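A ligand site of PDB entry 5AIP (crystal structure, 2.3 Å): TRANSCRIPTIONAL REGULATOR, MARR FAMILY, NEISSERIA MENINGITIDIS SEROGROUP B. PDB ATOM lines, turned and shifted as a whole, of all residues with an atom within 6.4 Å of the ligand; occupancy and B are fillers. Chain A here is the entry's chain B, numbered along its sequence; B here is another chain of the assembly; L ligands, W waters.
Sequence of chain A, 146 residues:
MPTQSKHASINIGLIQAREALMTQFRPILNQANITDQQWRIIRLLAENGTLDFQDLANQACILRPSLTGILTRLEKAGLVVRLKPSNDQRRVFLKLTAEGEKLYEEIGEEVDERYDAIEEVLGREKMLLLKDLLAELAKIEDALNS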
ATOM      1  N   ARG A  18       2.042 -13.721 -15.324  1.00  0.00           N
ATOM      2  CA  ARG A  18       1.475 -14.752 -14.465  1.00  0.00           C
ATOM      3  C   ARG A  18       2.520 -15.428 -13.593  1.00  0.00           C
ATOM      4  O   ARG A  18       2.286 -15.672 -12.415  1.00  0.00           O
ATOM      5  CB  ARG A  18       0.793 -15.833 -15.310  1.00  0.00           C
ATOM      6  CG  ARG A  18       0.072 -16.854 -14.473  1.00  0.00           C
ATOM      7  CD  ARG A  18      -0.405 -18.029 -15.296  1.00  0.00           C
ATOM      8  NE  ARG A  18      -0.653 -19.193 -14.449  1.00  0.00           N
ATOM      9  CZ  ARG A  18      -0.622 -20.450 -14.874  1.00  0.00           C
ATOM     10  NH1 ARG A  18      -0.346 -20.727 -16.147  1.00  0.00           N
ATOM     11  NH2 ARG A  18      -0.855 -21.438 -14.023  1.00  0.00           N
ATOM     12  N   LEU A  21       3.245 -13.233 -10.691  1.00  0.00           N
ATOM     13  CA  LEU A  21       2.217 -13.280  -9.653  1.00  0.00           C
ATOM     14  C   LEU A  21       2.351 -14.502  -8.776  1.00  0.00           C
ATOM     15  O   LEU A  21       2.222 -14.439  -7.553  1.00  0.00           O
ATOM     16  CB  LEU A  21       0.826 -13.282 -10.256  1.00  0.00           C
ATOM     17  CG  LEU A  21       0.271 -11.966 -10.764  1.00  0.00           C
ATOM     18  CD1 LEU A  21      -1.181 -12.220 -11.154  1.00  0.00           C
ATOM     19  CD2 LEU A  21       0.387 -10.915  -9.678  1.00  0.00           C
ATOM     20  N   MET A  22       2.605 -15.619  -9.446  1.00  0.00           N
ATOM     21  CA  MET A  22       2.834 -16.898  -8.798  1.00  0.00           C
ATOM     22  C   MET A  22       3.878 -16.825  -7.685  1.00  0.00           C
ATOM     23  O   MET A  22       3.681 -17.384  -6.611  1.00  0.00           O
ATOM     24  CB  MET A  22       3.266 -17.896  -9.866  1.00  0.00           C
ATOM     25  CG  MET A  22       3.169 -19.346  -9.477  1.00  0.00           C
ATOM     26  SD  MET A  22       3.834 -20.420 -10.956  1.00  0.00           S
ATOM     27  CE  MET A  22       2.925 -22.108 -10.531  1.00  0.00           C
ATOM     28  N   THR A  23       4.990 -16.149  -7.955  1.00  0.00           N
ATOM     29  CA  THR A  23       6.062 -16.038  -6.975  1.00  0.00           C
ATOM     30  C   THR A  23       5.632 -15.219  -5.763  1.00  0.00           C
ATOM     31  O   THR A  23       6.070 -15.458  -4.652  1.00  0.00           O
ATOM     32  CB  THR A  23       7.316 -15.373  -7.578  1.00  0.00           C
ATOM     33  OG1 THR A  23       7.092 -13.961  -7.690  1.00  0.00           O
ATOM     34  CG2 THR A  23       7.611 -15.940  -8.944  1.00  0.00           C
ATOM     35  N   PHE A  25       2.503 -15.148  -4.667  1.00  0.00           N
ATOM     36  CA  PHE A  25       1.441 -15.856  -3.938  1.00  0.00           C
ATOM     37  C   PHE A  25       1.803 -17.259  -3.522  1.00  0.00           C
ATOM     38  O   PHE A  25       1.133 -17.833  -2.670  1.00  0.00           O
ATOM     39  CB  PHE A  25       0.145 -15.856  -4.757  1.00  0.00           C
ATOM     40  CG  PHE A  25      -0.475 -14.497  -4.864  1.00  0.00           C
ATOM     41  CD1 PHE A  25      -1.313 -14.033  -3.876  1.00  0.00           C
ATOM     42  CD2 PHE A  25      -0.183 -13.666  -5.937  1.00  0.00           C
ATOM     43  CE1 PHE A  25      -1.877 -12.793  -3.958  1.00  0.00           C
ATOM     44  CE2 PHE A  25      -0.744 -12.424  -6.029  1.00  0.00           C
ATOM     45  CZ  PHE A  25      -1.594 -11.972  -5.037  1.00  0.00           C
ATOM     46  N   ARG A  26       2.888 -17.779  -4.082  1.00  0.00           N
ATOM     47  CA  ARG A  26       3.362 -19.130  -3.743  1.00  0.00           C
ATOM     48  C   ARG A  26       3.500 -19.370  -2.252  1.00  0.00           C
ATOM     49  O   ARG A  26       3.036 -20.392  -1.768  1.00  0.00           O
ATOM     50  CB  ARG A  26       4.720 -19.406  -4.397  1.00  0.00           C
ATOM     51  CG  ARG A  26       5.244 -20.811  -4.117  1.00  0.00           C
ATOM     52  CD  ARG A  26       6.382 -21.209  -5.033  1.00  0.00           C
ATOM     53  NE  ARG A  26       5.922 -21.487  -6.382  1.00  0.00           N
ATOM     54  CZ  ARG A  26       6.699 -21.462  -7.464  1.00  0.00           C
ATOM     55  NH1 ARG A  26       7.987 -21.164  -7.354  1.00  0.00           N
ATOM     56  NH2 ARG A  26       6.188 -21.734  -8.657  1.00  0.00           N
ATOM     57  N   LEU A  29      -0.007 -19.861  -0.696  1.00  0.00           N
ATOM     58  CA  LEU A  29      -0.681 -21.123  -1.024  1.00  0.00           C
ATOM     59  C   LEU A  29       0.042 -22.337  -0.418  1.00  0.00           C
ATOM     60  O   LEU A  29      -0.617 -23.280   0.023  1.00  0.00           O
ATOM     61  CB  LEU A  29      -0.803 -21.307  -2.542  1.00  0.00           C
ATOM     62  CG  LEU A  29      -1.727 -20.346  -3.292  1.00  0.00           C
ATOM     63  CD1 LEU A  29      -1.909 -20.822  -4.727  1.00  0.00           C
ATOM     64  CD2 LEU A  29      -3.070 -20.188  -2.596  1.00  0.00           C
ATOM     65  N   ASP A  36      -1.705 -24.143  -6.991  1.00  0.00           N
ATOM     66  CA  ASP A  36      -2.286 -23.057  -7.792  1.00  0.00           C
ATOM     67  C   ASP A  36      -3.614 -23.495  -8.430  1.00  0.00           C
ATOM     68  O   ASP A  36      -4.591 -22.732  -8.450  1.00  0.00           O
ATOM     69  CB  ASP A  36      -1.298 -22.574  -8.886  1.00  0.00           C
ATOM     70  CG  ASP A  36      -1.942 -21.559  -9.869  1.00  0.00           C
ATOM     71  OD1 ASP A  36      -2.853 -20.795  -9.481  1.00  0.00           O
ATOM     72  OD2 ASP A  36      -1.516 -21.531 -11.047  1.00  0.00           O
ATOM     73  N   TRP A  39      -6.390 -23.869  -5.823  1.00  0.00           N
ATOM     74  CA  TRP A  39      -6.833 -22.553  -5.406  1.00  0.00           C
ATOM     75  C   TRP A  39      -7.670 -21.898  -6.501  1.00  0.00           C
ATOM     76  O   TRP A  39      -8.667 -21.220  -6.231  1.00  0.00           O
ATOM     77  CB  TRP A  39      -5.640 -21.666  -5.051  1.00  0.00           C
ATOM     78  CG  TRP A  39      -6.015 -20.242  -4.780  1.00  0.00           C
ATOM     79  CD1 TRP A  39      -5.592 -19.131  -5.455  1.00  0.00           C
ATOM     80  CD2 TRP A  39      -6.944 -19.773  -3.780  1.00  0.00           C
ATOM     81  NE1 TRP A  39      -6.161 -18.000  -4.920  1.00  0.00           N
ATOM     82  CE2 TRP A  39      -6.994 -18.364  -3.894  1.00  0.00           C
ATOM     83  CE3 TRP A  39      -7.705 -20.407  -2.791  1.00  0.00           C
ATOM     84  CZ2 TRP A  39      -7.801 -17.580  -3.059  1.00  0.00           C
ATOM     85  CZ3 TRP A  39      -8.498 -19.630  -1.964  1.00  0.00           C
ATOM     86  CH2 TRP A  39      -8.539 -18.226  -2.098  1.00  0.00           C
ATOM     87  N   ARG A  43     -11.541 -20.725  -5.913  1.00  0.00           N
ATOM     88  CA  ARG A  43     -11.997 -19.362  -6.189  1.00  0.00           C
ATOM     89  C   ARG A  43     -13.170 -19.336  -7.163  1.00  0.00           C
ATOM     90  O   ARG A  43     -14.124 -18.576  -6.967  1.00  0.00           O
ATOM     91  CB  ARG A  43     -10.886 -18.490  -6.752  1.00  0.00           C
ATOM     92  CG  ARG A  43      -9.780 -18.201  -5.816  1.00  0.00           C
ATOM     93  CD  ARG A  43      -9.016 -16.997  -6.310  1.00  0.00           C
ATOM     94  NE  ARG A  43      -9.886 -15.835  -6.338  1.00  0.00           N
ATOM     95  CZ  ARG A  43      -9.470 -14.591  -6.198  1.00  0.00           C
ATOM     96  NH1 ARG A  43      -8.169 -14.342  -6.029  1.00  0.00           N
ATOM     97  NH2 ARG A  43     -10.338 -13.595  -6.221  1.00  0.00           N
ATOM     98  N   VAL A 111      -4.500 -13.485   0.422  1.00  0.00           N
ATOM     99  CA  VAL A 111      -4.332 -13.218  -1.004  1.00  0.00           C
ATOM    100  C   VAL A 111      -4.662 -11.750  -1.295  1.00  0.00           C
ATOM    101  O   VAL A 111      -3.943 -11.109  -2.069  1.00  0.00           O
ATOM    102  CB  VAL A 111      -5.233 -14.154  -1.873  1.00  0.00           C
ATOM    103  CG1 VAL A 111      -5.266 -13.688  -3.327  1.00  0.00           C
ATOM    104  CG2 VAL A 111      -4.696 -15.574  -1.844  1.00  0.00           C
ATOM    105  N   TYR A 115      -2.149  -8.751  -2.817  1.00  0.00           N
ATOM    106  CA  TYR A 115      -2.599  -7.881  -3.904  1.00  0.00           C
ATOM    107  C   TYR A 115      -2.526  -6.400  -3.552  1.00  0.00           C
ATOM    108  O   TYR A 115      -2.210  -5.573  -4.410  1.00  0.00           O
ATOM    109  CB  TYR A 115      -4.035  -8.227  -4.342  1.00  0.00           C
ATOM    110  CG  TYR A 115      -4.134  -9.267  -5.420  1.00  0.00           C
ATOM    111  CD1 TYR A 115      -3.539  -9.058  -6.657  1.00  0.00           C
ATOM    112  CD2 TYR A 115      -4.845 -10.451  -5.229  1.00  0.00           C
ATOM    113  CE1 TYR A 115      -3.626 -10.003  -7.675  1.00  0.00           C
ATOM    114  CE2 TYR A 115      -4.945 -11.399  -6.242  1.00  0.00           C
ATOM    115  CZ  TYR A 115      -4.325 -11.168  -7.465  1.00  0.00           C
ATOM    116  OH  TYR A 115      -4.415 -12.103  -8.481  1.00  0.00           O
ATOM    117  N   ALA B   8     -10.233  -9.104  -7.412  1.00  0.00           N
ATOM    118  CA  ALA B   8     -10.481 -10.118  -8.418  1.00  0.00           C
ATOM    119  C   ALA B   8      -9.146 -10.804  -8.750  1.00  0.00           C
ATOM    120  O   ALA B   8      -8.095 -10.200  -8.602  1.00  0.00           O
ATOM    121  CB  ALA B   8     -11.098  -9.485  -9.656  1.00  0.00           C
ATOM    122  N   SER B   9      -9.199 -12.051  -9.182  1.00  0.00           N
ATOM    123  CA  SER B   9      -7.977 -12.774  -9.521  1.00  0.00           C
ATOM    124  C   SER B   9      -7.414 -12.335 -10.869  1.00  0.00           C
ATOM    125  O   SER B   9      -7.938 -12.674 -11.929  1.00  0.00           O
ATOM    126  CB  SER B   9      -8.234 -14.271  -9.541  1.00  0.00           C
ATOM    127  OG  SER B   9      -7.070 -14.952  -9.990  1.00  0.00           O
ATOM    128  N   ILE B  10      -6.344 -11.554 -10.836  1.00  0.00           N
ATOM    129  CA  ILE B  10      -5.653 -11.158 -12.060  1.00  0.00           C
ATOM    130  C   ILE B  10      -5.056 -12.412 -12.689  1.00  0.00           C
ATOM    131  O   ILE B  10      -4.927 -12.528 -13.902  1.00  0.00           O
ATOM    132  CB  ILE B  10      -4.585 -10.091 -11.785  1.00  0.00           C
ATOM    133  CG1 ILE B  10      -5.245  -8.837 -11.212  1.00  0.00           C
ATOM    134  CG2 ILE B  10      -3.806  -9.739 -13.030  1.00  0.00           C
ATOM    135  CD1 ILE B  10      -4.261  -7.955 -10.433  1.00  0.00           C
ATOM    136  N   ASN B  11      -4.661 -13.342 -11.833  1.00  0.00           N
ATOM    137  CA  ASN B  11      -4.099 -14.616 -12.262  1.00  0.00           C
ATOM    138  C   ASN B  11      -5.034 -15.340 -13.258  1.00  0.00           C
ATOM    139  O   ASN B  11      -4.626 -15.689 -14.357  1.00  0.00           O
ATOM    140  CB  ASN B  11      -3.841 -15.505 -11.064  1.00  0.00           C
ATOM    141  CG  ASN B  11      -3.153 -16.797 -11.451  1.00  0.00           C
ATOM    142  OD1 ASN B  11      -2.223 -16.785 -12.260  1.00  0.00           O
ATOM    143  ND2 ASN B  11      -3.628 -17.912 -10.916  1.00  0.00           N
ATOM    144  N   ILE B  12      -6.287 -15.550 -12.843  1.00  0.00           N
ATOM    145  CA  ILE B  12      -7.256 -16.214 -13.685  1.00  0.00           C
ATOM    146  C   ILE B  12      -7.483 -15.387 -14.973  1.00  0.00           C
ATOM    147  O   ILE B  12      -7.624 -15.949 -16.052  1.00  0.00           O
ATOM    148  CB  ILE B  12      -8.604 -16.446 -12.940  1.00  0.00           C
ATOM    149  CG1 ILE B  12      -8.455 -17.482 -11.817  1.00  0.00           C
ATOM    150  CG2 ILE B  12      -9.689 -16.899 -13.917  1.00  0.00           C
ATOM    151  CD1 ILE B  12      -9.654 -17.559 -10.882  1.00  0.00           C
HETATM  152  C1  LIG L   1      -4.897 -15.152  -7.125  1.00  0.00           C
HETATM  153  O1  LIG L   1      -5.887 -15.765  -6.631  1.00  0.00           O
HETATM  154  O2  LIG L   1      -5.011 -14.515  -8.219  1.00  0.00           O
HETATM  155  C2  LIG L   1      -3.580 -15.170  -6.412  1.00  0.00           C
HETATM  156  C3  LIG L   1      -2.638 -16.089  -7.120  1.00  0.00           C
HETATM  157  C4  LIG L   1      -2.525 -17.523  -6.693  1.00  0.00           C
HETATM  158  C5  LIG L   1      -1.663 -18.364  -7.325  1.00  0.00           C
HETATM  159  C6  LIG L   1      -0.841 -17.869  -8.465  1.00  0.00           C
HETATM  160  C7  LIG L   1      -0.943 -16.562  -8.863  1.00  0.00           C
HETATM  161  C8  LIG L   1      -1.876 -15.643  -8.152  1.00  0.00           C
HETATM  162  O3  LIG L   1       0.024 -18.730  -9.100  1.00  0.00           O
HETATM  163  O   HOH W   1      -5.780 -17.944  -8.522  1.00  0.00           O
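The backbone NH (N) of Ile 12 of chain B is in hydrogen-bond range of the side-chain hydroxyl (OG) of Ser 9 of chain B (3.0 Å). OD2 of Asp 36 lies within salt-bridge range of NH2 of Arg 18 (3.0 Å). SD of Met 22 lies within hydrogen-bond range of NH2 of Arg 26 (3.5 Å). N of Asn 11 of chain B sits close to OG of Ser 9 of chain B (3.4 Å). The side-chain hydroxyl (OH) of Tyr 115 is in hydrogen-bond range of the backbone NH (N) of Ile 10 of chain B (3.1 Å). OD1 of Asp 36 sits at hydrogen-bond distance from ND2 of Asn 11 of chain B, 3.3 Å away.
O1 of the ligand is in hydrogen-bond range of NE1 of Trp 39. O2 of the ligand is in hydrogen-bond range of OG of Ser 9 of chain B (2.8 Å). The guanidinium group of Arg 43 is in salt-bridge range of an oxygen (O1) of the ligand (2.8 Å). The side-chain hydroxyl (OH) of Tyr 115 sits at hydrogen-bond distance from an oxygen (O2) of the ligand.
Leu 21 touches the ligand (C to C7, 3.9 Å). CG of Met 22 touches O3 of the ligand (3.2 Å). Phe 25 touches the ligand (CD2 to C8, 3.4 Å). CD1 of Leu 29 touches C5 of the ligand (3.6 Å). Asp 36 touches the ligand. CG1 of Val 111 touches C2 of the ligand, at 3.8 Å. Asn 11 of chain B touches the ligand (CB to O2, 3.2 Å). Hydrophobic or aromatic side chains within 4 Å of the ligand: Leu 21, Met 22, Phe 25, Leu 29, Trp 39, Val 111 and Tyr 115. Within 4 Å of the ligand: Leu 21, Met 22, Phe 25, Leu 29, Asp 36, Trp 39, Arg 43, Val 111, Tyr 115, Ser 9 of chain B and Asn 11 of chain B.
Water W1 lies within hydrogen-bond range of an oxygen (O1) of the ligand and the side-chain amide nitrogen (ND2) of Asn 11 of chain B.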
